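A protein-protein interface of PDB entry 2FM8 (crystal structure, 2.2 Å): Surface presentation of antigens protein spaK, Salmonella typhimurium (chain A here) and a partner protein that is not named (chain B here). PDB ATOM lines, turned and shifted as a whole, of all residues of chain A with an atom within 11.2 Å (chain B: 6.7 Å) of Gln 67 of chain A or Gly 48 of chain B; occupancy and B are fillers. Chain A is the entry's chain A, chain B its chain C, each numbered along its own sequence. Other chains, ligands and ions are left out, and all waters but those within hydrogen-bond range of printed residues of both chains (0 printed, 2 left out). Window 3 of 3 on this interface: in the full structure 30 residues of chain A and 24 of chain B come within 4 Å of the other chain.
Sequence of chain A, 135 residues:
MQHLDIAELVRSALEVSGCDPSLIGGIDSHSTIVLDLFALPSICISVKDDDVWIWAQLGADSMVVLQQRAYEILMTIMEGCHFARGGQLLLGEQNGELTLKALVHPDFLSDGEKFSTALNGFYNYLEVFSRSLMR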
ATOM      1  N   GLY A  59       9.531 -27.492  -1.459  1.00  0.00           N
ATOM      2  CA  GLY A  59      10.431 -26.740  -0.573  1.00  0.00           C
ATOM      3  C   GLY A  59      10.610 -25.278  -0.955  1.00  0.00           C
ATOM      4  O   GLY A  59      10.461 -24.899  -2.126  1.00  0.00           O
ATOM      5  N   ALA A  60      10.913 -24.465   0.057  1.00  0.00           N
ATOM      6  CA  ALA A  60      11.009 -22.998  -0.079  1.00  0.00           C
ATOM      7  C   ALA A  60      11.991 -22.554  -1.163  1.00  0.00           C
ATOM      8  O   ALA A  60      11.774 -21.537  -1.814  1.00  0.00           O
ATOM      9  CB  ALA A  60      11.415 -22.372   1.267  1.00  0.00           C
ATOM     10  N   ASP A  61      13.076 -23.292  -1.342  1.00  0.00           N
ATOM     11  CA  ASP A  61      14.088 -22.918  -2.351  1.00  0.00           C
ATOM     12  C   ASP A  61      14.040 -23.729  -3.652  1.00  0.00           C
ATOM     13  O   ASP A  61      14.934 -23.591  -4.481  1.00  0.00           O
ATOM     14  CB  ASP A  61      15.486 -23.064  -1.756  1.00  0.00           C
ATOM     15  CG  ASP A  61      15.778 -22.016  -0.676  1.00  0.00           C
ATOM     16  OD1 ASP A  61      15.200 -20.884  -0.726  1.00  0.00           O
ATOM     17  OD2 ASP A  61      16.614 -22.328   0.199  1.00  0.00           O
ATOM     18  N   SER A  62      13.006 -24.549  -3.824  1.00  0.00           N
ATOM     19  CA  SER A  62      12.936 -25.472  -4.964  1.00  0.00           C
ATOM     20  C   SER A  62      12.983 -24.746  -6.326  1.00  0.00           C
ATOM     21  O   SER A  62      13.643 -25.227  -7.246  1.00  0.00           O
ATOM     22  CB  SER A  62      11.695 -26.393  -4.872  1.00  0.00           C
ATOM     23  OG  SER A  62      10.500 -25.660  -4.652  1.00  0.00           O
ATOM     24  N   MET A  63      12.325 -23.602  -6.459  1.00  0.00           N
ATOM     25  CA  MET A  63      12.300 -22.917  -7.769  1.00  0.00           C
ATOM     26  C   MET A  63      13.693 -22.387  -8.147  1.00  0.00           C
ATOM     27  O   MET A  63      14.104 -22.465  -9.286  1.00  0.00           O
ATOM     28  CB  MET A  63      11.262 -21.807  -7.809  1.00  0.00           C
ATOM     29  CG  MET A  63       9.804 -22.310  -7.762  1.00  0.00           C
ATOM     30  SD  MET A  63       9.264 -23.300  -9.176  1.00  0.00           S
ATOM     31  CE  MET A  63       9.362 -22.148 -10.543  1.00  0.00           C
ATOM     32  N   VAL A  64      14.422 -21.879  -7.163  1.00  0.00           N
ATOM     33  CA  VAL A  64      15.794 -21.436  -7.357  1.00  0.00           C
ATOM     34  C   VAL A  64      16.722 -22.624  -7.679  1.00  0.00           C
ATOM     35  O   VAL A  64      17.498 -22.576  -8.635  1.00  0.00           O
ATOM     36  CB  VAL A  64      16.270 -20.644  -6.131  1.00  0.00           C
ATOM     37  CG1 VAL A  64      17.792 -20.493  -6.089  1.00  0.00           C
ATOM     38  CG2 VAL A  64      15.565 -19.282  -6.110  1.00  0.00           C
ATOM     39  N   VAL A  65      16.634 -23.702  -6.914  1.00  0.00           N
ATOM     40  CA  VAL A  65      17.513 -24.828  -7.185  1.00  0.00           C
ATOM     41  C   VAL A  65      17.209 -25.399  -8.567  1.00  0.00           C
ATOM     42  O   VAL A  65      18.117 -25.856  -9.268  1.00  0.00           O
ATOM     43  CB  VAL A  65      17.430 -25.911  -6.106  1.00  0.00           C
ATOM     44  CG1 VAL A  65      18.314 -27.078  -6.469  1.00  0.00           C
ATOM     45  CG2 VAL A  65      17.871 -25.324  -4.733  1.00  0.00           C
ATOM     46  N   LEU A  66      15.931 -25.341  -8.968  1.00  0.00           N
ATOM     47  CA  LEU A  66      15.522 -25.766 -10.310  1.00  0.00           C
ATOM     48  C   LEU A  66      16.342 -25.093 -11.443  1.00  0.00           C
ATOM     49  O   LEU A  66      16.583 -25.694 -12.487  1.00  0.00           O
ATOM     50  CB  LEU A  66      14.033 -25.565 -10.498  1.00  0.00           C
ATOM     51  CG  LEU A  66      13.368 -26.136 -11.765  1.00  0.00           C
ATOM     52  CD1 LEU A  66      13.497 -27.656 -11.892  1.00  0.00           C
ATOM     53  CD2 LEU A  66      11.923 -25.747 -11.773  1.00  0.00           C
ATOM     54  N   GLN A  67      16.788 -23.867 -11.223  1.00  0.00           N
ATOM     55  CA  GLN A  67      17.621 -23.152 -12.202  1.00  0.00           C
ATOM     56  C   GLN A  67      18.910 -23.904 -12.573  1.00  0.00           C
ATOM     57  O   GLN A  67      19.428 -23.745 -13.659  1.00  0.00           O
ATOM     58  CB  GLN A  67      17.971 -21.743 -11.691  1.00  0.00           C
ATOM     59  CG  GLN A  67      16.758 -20.887 -11.322  1.00  0.00           C
ATOM     60  CD  GLN A  67      17.123 -19.578 -10.702  1.00  0.00           C
ATOM     61  OE1 GLN A  67      18.228 -19.028 -10.935  1.00  0.00           O
ATOM     62  NE2 GLN A  67      16.199 -19.032  -9.930  1.00  0.00           N
ATOM     63  N   GLN A  68      19.423 -24.706 -11.652  1.00  0.00           N
ATOM     64  CA  GLN A  68      20.636 -25.466 -11.870  1.00  0.00           C
ATOM     65  C   GLN A  68      20.366 -26.938 -12.136  1.00  0.00           C
ATOM     66  O   GLN A  68      21.234 -27.615 -12.632  1.00  0.00           O
ATOM     67  CB  GLN A  68      21.545 -25.374 -10.637  1.00  0.00           C
ATOM     68  CG  GLN A  68      22.329 -24.081 -10.524  1.00  0.00           C
ATOM     69  CD  GLN A  68      23.107 -24.007  -9.192  1.00  0.00           C
ATOM     70  OE1 GLN A  68      23.342 -25.038  -8.528  1.00  0.00           O
ATOM     71  NE2 GLN A  68      23.496 -22.794  -8.795  1.00  0.00           N
ATOM     72  N   ARG A  69      19.180 -27.430 -11.785  1.00  0.00           N
ATOM     73  CA  ARG A  69      18.891 -28.872 -11.813  1.00  0.00           C
ATOM     74  C   ARG A  69      17.788 -29.293 -12.757  1.00  0.00           C
ATOM     75  O   ARG A  69      17.276 -30.428 -12.666  1.00  0.00           O
ATOM     76  CB  ARG A  69      18.573 -29.349 -10.401  1.00  0.00           C
ATOM     77  CG  ARG A  69      19.729 -30.036  -9.759  1.00  0.00           C
ATOM     78  CD  ARG A  69      20.444 -29.175  -8.831  1.00  0.00           C
ATOM     79  NE  ARG A  69      21.790 -29.696  -8.621  1.00  0.00           N
ATOM     80  CZ  ARG A  69      22.453 -29.634  -7.457  1.00  0.00           C
ATOM     81  NH1 ARG A  69      21.894 -29.068  -6.342  1.00  0.00           N
ATOM     82  NH2 ARG A  69      23.697 -30.162  -7.403  1.00  0.00           N
ATOM     83  N   ALA A  70      17.407 -28.404 -13.672  1.00  0.00           N
ATOM     84  CA  ALA A  70      16.284 -28.683 -14.555  1.00  0.00           C
ATOM     85  C   ALA A  70      16.489 -29.899 -15.455  1.00  0.00           C
ATOM     86  O   ALA A  70      15.534 -30.642 -15.696  1.00  0.00           O
ATOM     87  CB  ALA A  70      15.912 -27.473 -15.381  1.00  0.00           C
ATOM     88  N   TYR A  71      17.706 -30.140 -15.921  1.00  0.00           N
ATOM     89  CA  TYR A  71      17.952 -31.323 -16.753  1.00  0.00           C
ATOM     90  C   TYR A  71      17.741 -32.648 -16.020  1.00  0.00           C
ATOM     91  O   TYR A  71      17.095 -33.574 -16.513  1.00  0.00           O
ATOM     92  CB  TYR A  71      19.380 -31.281 -17.265  1.00  0.00           C
ATOM     93  CG  TYR A  71      19.752 -32.407 -18.186  1.00  0.00           C
ATOM     94  CD1 TYR A  71      18.943 -32.748 -19.297  1.00  0.00           C
ATOM     95  CD2 TYR A  71      20.914 -33.135 -17.962  1.00  0.00           C
ATOM     96  CE1 TYR A  71      19.307 -33.784 -20.151  1.00  0.00           C
ATOM     97  CE2 TYR A  71      21.283 -34.154 -18.799  1.00  0.00           C
ATOM     98  CZ  TYR A  71      20.496 -34.474 -19.893  1.00  0.00           C
ATOM     99  OH  TYR A  71      20.941 -35.470 -20.708  1.00  0.00           O
ATOM    100  N   GLU A  72      18.313 -32.737 -14.825  1.00  0.00           N
ATOM    101  CA  GLU A  72      18.125 -33.910 -13.978  1.00  0.00           C
ATOM    102  C   GLU A  72      16.638 -34.119 -13.650  1.00  0.00           C
ATOM    103  O   GLU A  72      16.146 -35.252 -13.592  1.00  0.00           O
ATOM    104  CB  GLU A  72      18.983 -33.766 -12.706  1.00  0.00           C
ATOM    105  CG  GLU A  72      18.705 -34.829 -11.642  1.00  0.00           C
ATOM    106  CD  GLU A  72      19.667 -34.716 -10.443  1.00  0.00           C
ATOM    107  OE1 GLU A  72      20.766 -34.191 -10.618  1.00  0.00           O
ATOM    108  OE2 GLU A  72      19.317 -35.139  -9.343  1.00  0.00           O
ATOM    109  N   ILE A  73      15.925 -33.030 -13.438  1.00  0.00           N
ATOM    110  CA  ILE A  73      14.506 -33.114 -13.133  1.00  0.00           C
ATOM    111  C   ILE A  73      13.733 -33.610 -14.343  1.00  0.00           C
ATOM    112  O   ILE A  73      12.899 -34.508 -14.233  1.00  0.00           O
ATOM    113  CB  ILE A  73      13.989 -31.766 -12.606  1.00  0.00           C
ATOM    114  CG1 ILE A  73      14.570 -31.493 -11.196  1.00  0.00           C
ATOM    115  CG2 ILE A  73      12.462 -31.689 -12.605  1.00  0.00           C
ATOM    116  CD1 ILE A  73      14.006 -32.383 -10.080  1.00  0.00           C
ATOM    117  N   LEU A  74      14.037 -33.056 -15.509  1.00  0.00           N
ATOM    118  CA  LEU A  74      13.401 -33.513 -16.740  1.00  0.00           C
ATOM    119  C   LEU A  74      13.657 -35.009 -17.059  1.00  0.00           C
ATOM    120  O   LEU A  74      12.732 -35.720 -17.459  1.00  0.00           O
ATOM    121  CB  LEU A  74      13.803 -32.620 -17.889  1.00  0.00           C
ATOM    122  CG  LEU A  74      12.772 -31.824 -18.682  1.00  0.00           C
ATOM    123  CD1 LEU A  74      11.487 -31.500 -17.990  1.00  0.00           C
ATOM    124  CD2 LEU A  74      13.444 -30.579 -19.246  1.00  0.00           C
ATOM    125  N   LEU A  91       4.697 -31.133 -13.122  1.00  0.00           N
ATOM    126  CA  LEU A  91       5.256 -30.122 -12.243  1.00  0.00           C
ATOM    127  C   LEU A  91       4.428 -28.855 -12.318  1.00  0.00           C
ATOM    128  O   LEU A  91       4.138 -28.373 -13.382  1.00  0.00           O
ATOM    129  CB  LEU A  91       6.694 -29.797 -12.634  1.00  0.00           C
ATOM    130  CG  LEU A  91       7.664 -30.947 -12.473  1.00  0.00           C
ATOM    131  CD1 LEU A  91       8.969 -30.609 -13.206  1.00  0.00           C
ATOM    132  CD2 LEU A  91       7.952 -31.251 -11.015  1.00  0.00           C
ATOM    133  N   GLU A  93       3.548 -25.113  -9.595  1.00  0.00           N
ATOM    134  CA  GLU A  93       4.097 -24.209  -8.614  1.00  0.00           C
ATOM    135  C   GLU A  93       2.989 -23.687  -7.676  1.00  0.00           C
ATOM    136  O   GLU A  93       2.005 -23.150  -8.123  1.00  0.00           O
ATOM    137  CB  GLU A  93       4.798 -23.030  -9.301  1.00  0.00           C
ATOM    138  CG  GLU A  93       5.487 -22.139  -8.259  1.00  0.00           C
ATOM    139  CD  GLU A  93       6.138 -20.916  -8.796  1.00  0.00           C
ATOM    140  OE1 GLU A  93       6.004 -20.635  -9.996  1.00  0.00           O
ATOM    141  OE2 GLU A  93       6.788 -20.221  -7.987  1.00  0.00           O
ATOM    142  N   GLY A  96       4.860 -20.222  -4.280  1.00  0.00           N
ATOM    143  CA  GLY A  96       6.264 -19.957  -4.655  1.00  0.00           C
ATOM    144  C   GLY A  96       7.175 -21.176  -4.603  1.00  0.00           C
ATOM    145  O   GLY A  96       8.393 -21.052  -4.579  1.00  0.00           O
ATOM    146  N   LEU A  98       8.020 -25.224  -6.173  1.00  0.00           N
ATOM    147  CA  LEU A  98       7.770 -26.236  -7.167  1.00  0.00           C
ATOM    148  C   LEU A  98       6.895 -27.362  -6.592  1.00  0.00           C
ATOM    149  O   LEU A  98       7.109 -27.820  -5.455  1.00  0.00           O
ATOM    150  CB  LEU A  98       9.074 -26.825  -7.665  1.00  0.00           C
ATOM    151  CG  LEU A  98       8.957 -27.717  -8.905  1.00  0.00           C
ATOM    152  CD1 LEU A  98       8.566 -26.911 -10.139  1.00  0.00           C
ATOM    153  CD2 LEU A  98      10.334 -28.361  -9.118  1.00  0.00           C
ATOM    154  N   SER A 132      16.844 -34.314  -5.544  1.00  0.00           N
ATOM    155  CA  SER A 132      17.405 -33.641  -6.713  1.00  0.00           C
ATOM    156  C   SER A 132      17.347 -32.109  -6.590  1.00  0.00           C
ATOM    157  O   SER A 132      18.108 -31.420  -7.276  1.00  0.00           O
ATOM    158  CB  SER A 132      16.701 -34.034  -8.023  1.00  0.00           C
ATOM    159  OG  SER A 132      16.987 -35.367  -8.384  1.00  0.00           O
ATOM    160  N   LEU A 133      16.431 -31.591  -5.771  1.00  0.00           N
ATOM    161  CA  LEU A 133      16.281 -30.129  -5.584  1.00  0.00           C
ATOM    162  C   LEU A 133      16.894 -29.605  -4.298  1.00  0.00           C
ATOM    163  O   LEU A 133      16.640 -28.480  -3.881  1.00  0.00           O
ATOM    164  CB  LEU A 133      14.825 -29.736  -5.657  1.00  0.00           C
ATOM    165  CG  LEU A 133      14.284 -29.861  -7.082  1.00  0.00           C
ATOM    166  CD1 LEU A 133      12.786 -29.972  -7.031  1.00  0.00           C
ATOM    167  CD2 LEU A 133      14.701 -28.718  -7.993  1.00  0.00           C
ATOM    168  N   MET A 134      17.743 -30.407  -3.694  1.00  0.00           N
ATOM    169  CA  MET A 134      18.395 -30.013  -2.476  1.00  0.00           C
ATOM    170  C   MET A 134      19.530 -29.081  -2.876  1.00  0.00           C
ATOM    171  O   MET A 134      20.223 -29.363  -3.865  1.00  0.00           O
ATOM    172  CB  MET A 134      18.934 -31.243  -1.743  1.00  0.00           C
ATOM    173  CG  MET A 134      18.850 -31.127  -0.265  1.00  0.00           C
ATOM    174  SD  MET A 134      19.367 -32.627   0.611  1.00  0.00           S
ATOM    175  CE  MET A 134      21.123 -32.529   0.156  1.00  0.00           C
ATOM    176  N   LEU B  44      18.693 -16.497 -19.741  1.00  0.00           N
ATOM    177  CA  LEU B  44      19.521 -15.539 -18.997  1.00  0.00           C
ATOM    178  C   LEU B  44      19.221 -15.562 -17.494  1.00  0.00           C
ATOM    179  O   LEU B  44      20.128 -15.636 -16.668  1.00  0.00           O
ATOM    180  CB  LEU B  44      19.291 -14.113 -19.536  1.00  0.00           C
ATOM    181  CG  LEU B  44      19.996 -12.981 -18.745  1.00  0.00           C
ATOM    182  CD1 LEU B  44      21.473 -13.158 -18.768  1.00  0.00           C
ATOM    183  CD2 LEU B  44      19.622 -11.627 -19.283  1.00  0.00           C
ATOM    184  N   PHE B  45      17.944 -15.441 -17.147  1.00  0.00           N
ATOM    185  CA  PHE B  45      17.542 -15.244 -15.750  1.00  0.00           C
ATOM    186  C   PHE B  45      17.884 -16.459 -14.867  1.00  0.00           C
ATOM    187  O   PHE B  45      18.038 -16.308 -13.640  1.00  0.00           O
ATOM    188  CB  PHE B  45      16.063 -14.902 -15.648  1.00  0.00           C
ATOM    189  CG  PHE B  45      15.692 -13.515 -16.161  1.00  0.00           C
ATOM    190  CD1 PHE B  45      16.634 -12.548 -16.448  1.00  0.00           C
ATOM    191  CD2 PHE B  45      14.335 -13.184 -16.331  1.00  0.00           C
ATOM    192  CE1 PHE B  45      16.238 -11.283 -16.891  1.00  0.00           C
ATOM    193  CE2 PHE B  45      13.950 -11.937 -16.768  1.00  0.00           C
ATOM    194  CZ  PHE B  45      14.894 -10.987 -17.038  1.00  0.00           C
ATOM    195  N   LYS B  46      18.033 -17.636 -15.492  1.00  0.00           N
ATOM    196  CA  LYS B  46      18.546 -18.834 -14.797  1.00  0.00           C
ATOM    197  C   LYS B  46      19.903 -18.581 -14.140  1.00  0.00           C
ATOM    198  O   LYS B  46      20.227 -19.251 -13.185  1.00  0.00           O
ATOM    199  CB  LYS B  46      18.621 -20.080 -15.718  1.00  0.00           C
ATOM    200  CG  LYS B  46      19.944 -20.348 -16.474  1.00  0.00           C
ATOM    201  CD  LYS B  46      20.062 -21.831 -16.958  1.00  0.00           C
ATOM    202  CE  LYS B  46      21.504 -22.386 -17.105  1.00  0.00           C
ATOM    203  NZ  LYS B  46      22.169 -22.384 -18.476  1.00  0.00           N
ATOM    204  N   CYS B  47      20.695 -17.643 -14.668  1.00  0.00           N
ATOM    205  CA  CYS B  47      22.016 -17.345 -14.106  1.00  0.00           C
ATOM    206  C   CYS B  47      21.945 -16.485 -12.861  1.00  0.00           C
ATOM    207  O   CYS B  47      22.931 -16.352 -12.179  1.00  0.00           O
ATOM    208  CB  CYS B  47      22.900 -16.627 -15.113  1.00  0.00           C
ATOM    209  SG  CYS B  47      23.106 -17.528 -16.620  1.00  0.00           S
ATOM    210  N   GLY B  48      20.804 -15.879 -12.592  1.00  0.00           N
ATOM    211  CA  GLY B  48      20.638 -15.071 -11.397  1.00  0.00           C
ATOM    212  C   GLY B  48      20.451 -15.839 -10.094  1.00  0.00           C
ATOM    213  O   GLY B  48      20.321 -17.063 -10.075  1.00  0.00           O
ATOM    214  N   LYS B  49      20.470 -15.107  -8.994  1.00  0.00           N
ATOM    215  CA  LYS B  49      20.212 -15.705  -7.675  1.00  0.00           C
ATOM    216  C   LYS B  49      18.775 -16.237  -7.611  1.00  0.00           C
ATOM    217  O   LYS B  49      18.545 -17.302  -7.083  1.00  0.00           O
ATOM    218  CB  LYS B  49      20.456 -14.684  -6.558  1.00  0.00           C
ATOM    219  CG  LYS B  49      21.931 -14.293  -6.420  1.00  0.00           C
ATOM    220  CD  LYS B  49      22.117 -13.273  -5.278  1.00  0.00           C
ATOM    221  CE  LYS B  49      23.600 -13.001  -4.859  1.00  0.00           C
ATOM    222  NZ  LYS B  49      23.808 -11.880  -3.805  1.00  0.00           N
ATOM    223  N   ASP B  50      17.848 -15.497  -8.211  1.00  0.00           N
ATOM    224  CA  ASP B  50      16.434 -15.806  -8.202  1.00  0.00           C
ATOM    225  C   ASP B  50      15.786 -15.353  -9.513  1.00  0.00           C
ATOM    226  O   ASP B  50      15.499 -14.163  -9.709  1.00  0.00           O
ATOM    227  CB  ASP B  50      15.785 -15.109  -7.001  1.00  0.00           C
ATOM    228  CG  ASP B  50      14.350 -15.504  -6.797  1.00  0.00           C
ATOM    229  OD1 ASP B  50      13.685 -15.878  -7.766  1.00  0.00           O
ATOM    230  OD2 ASP B  50      13.871 -15.429  -5.653  1.00  0.00           O
ATOM    231  N   ALA B  51      15.579 -16.305 -10.421  1.00  0.00           N
ATOM    232  CA  ALA B  51      14.961 -16.033 -11.729  1.00  0.00           C
ATOM    233  C   ALA B  51      13.576 -15.393 -11.644  1.00  0.00           C
ATOM    234  O   ALA B  51      13.232 -14.517 -12.457  1.00  0.00           O
ATOM    235  CB  ALA B  51      14.881 -17.307 -12.536  1.00  0.00           C
ATOM    236  N   GLU B  52      12.767 -15.830 -10.678  1.00  0.00           N
ATOM    237  CA  GLU B  52      11.417 -15.270 -10.504  1.00  0.00           C
ATOM    238  C   GLU B  52      11.480 -13.791 -10.128  1.00  0.00           C
ATOM    239  O   GLU B  52      10.692 -12.978 -10.616  1.00  0.00           O
ATOM    240  CB  GLU B  52      10.623 -16.041  -9.447  1.00  0.00           C
ATOM    241  CG  GLU B  52      10.200 -17.459  -9.867  1.00  0.00           C
ATOM    242  CD  GLU B  52       9.295 -18.159  -8.816  1.00  0.00           C
ATOM    243  OE1 GLU B  52       9.725 -18.406  -7.647  1.00  0.00           O
ATOM    244  OE2 GLU B  52       8.128 -18.447  -9.168  1.00  0.00           O
ATOM    245  N   LEU B  54      13.854 -11.772 -10.934  1.00  0.00           N
ATOM    246  CA  LEU B  54      14.290 -11.067 -12.141  1.00  0.00           C
ATOM    247  C   LEU B  54      13.091 -10.785 -13.067  1.00  0.00           C
ATOM    248  O   LEU B  54      12.903  -9.664 -13.564  1.00  0.00           O
ATOM    249  CB  LEU B  54      15.358 -11.882 -12.844  1.00  0.00           C
ATOM    250  CG  LEU B  54      16.749 -11.736 -12.204  1.00  0.00           C
ATOM    251  CD1 LEU B  54      17.639 -12.914 -12.561  1.00  0.00           C
ATOM    252  CD2 LEU B  54      17.427 -10.410 -12.651  1.00  0.00           C
ATOM    253  N   GLY B  98      26.738 -13.881 -17.040  1.00  0.00           N
ATOM    254  CA  GLY B  98      25.307 -14.013 -16.721  1.00  0.00           C
ATOM    255  C   GLY B  98      24.947 -13.625 -15.306  1.00  0.00           C
ATOM    256  O   GLY B  98      24.000 -12.864 -15.058  1.00  0.00           O
ATOM    257  N   ALA B  99      25.727 -14.121 -14.361  1.00  0.00           N
ATOM    258  CA  ALA B  99      25.481 -13.823 -12.959  1.00  0.00           C
ATOM    259  C   ALA B  99      25.700 -12.365 -12.667  1.00  0.00           C
ATOM    260  O   ALA B  99      24.953 -11.735 -11.904  1.00  0.00           O
ATOM    261  CB  ALA B  99      26.371 -14.686 -12.074  1.00  0.00           C
ATOM    262  N   THR B 102      22.799 -10.196 -14.421  1.00  0.00           N
ATOM    263  CA  THR B 102      21.544 -10.345 -13.673  1.00  0.00           C
ATOM    264  C   THR B 102      21.571  -9.712 -12.288  1.00  0.00           C
ATOM    265  O   THR B 102      20.576  -9.117 -11.875  1.00  0.00           O
ATOM    266  CB  THR B 102      21.079 -11.820 -13.559  1.00  0.00           C
ATOM    267  OG1 THR B 102      22.128 -12.637 -13.016  1.00  0.00           O
ATOM    268  CG2 THR B 102      20.677 -12.329 -14.895  1.00  0.00           C
ATOM    269  N   ALA B 103      22.692  -9.818 -11.582  1.00  0.00           N
ATOM    270  CA  ALA B 103      22.842  -9.145 -10.302  1.00  0.00           C
ATOM    271  C   ALA B 103      22.722  -7.641 -10.427  1.00  0.00           C
ATOM    272  O   ALA B 103      22.236  -6.975  -9.505  1.00  0.00           O
ATOM    273  CB  ALA B 103      24.190  -9.506  -9.636  1.00  0.00           C
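OE1 of Gln 67 of chain A sits close to O of Lys 46 of chain B (3.0 Å).
The side-chain carboxylate of Glu 52 of chain B sits close to the side-chain carboxylate of Glu 93 of chain A.
OE1 of Gln 67 of chain A sits close to O of Gly 48 of chain B (3.0 Å).
NE2 of Gln 67 of chain A lies close to N of Ala 51 of chain B (2.8 Å).
The side-chain carboxylate of Asp 50 of chain B sits at hydrogen-bond distance from the backbone NH of Glu 52 of chain B (3.1 Å).
N of Leu 98 of chain A sits close to SD of Met 63 of chain A (3.8 Å).
Among the printed residues, merely in contact across the chains: Met 63 of chain A with Glu 52 of chain B (3.7 Å), Val 64 of chain A with Lys 49 of chain B (3.4 Å), Gln 67 of chain A with Phe 45 of chain B (3.8 Å) and Gln 67 of chain A with Asp 50 of chain B (3.7 Å).
Gln 67 of chain A touches five residues of chain B.
Arg 69 of chain A touches none of the printed residues of chain B.
Of the printed residues of chain B, Glu 93 of chain A touches Glu 52.
Of chain A, only Gln 67 (3.0 Å) comes within 4 Å of Lys 46 of chain B.
No residue of chain A comes within 4 Å of Cys 47 of chain B.
Of chain A, only Gln 67 comes within 4 Å of Gly 48 of chain B.
Printed residues of chain A within 4 Å of Lys 49 of chain B: Val 64.
The nearest residue of chain A that does not touch Gly 48 of chain B is Val 64 of chain A (5.8 Å).
The nearest printed residue of chain B that does not touch Val 64 of chain A is Asp 50 of chain B (4.03 Å).
Printed residues of chain B that touch a printed residue of chain A: Phe 45, Lys 46, Gly 48, Lys 49, Asp 50, Ala 51 and Glu 52.
Of the 23 printed residues of chain A, 4 touch a printed residue of chain B.
Along chain A the printed residues that touch a printed residue of chain B span positions 63 to 93.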
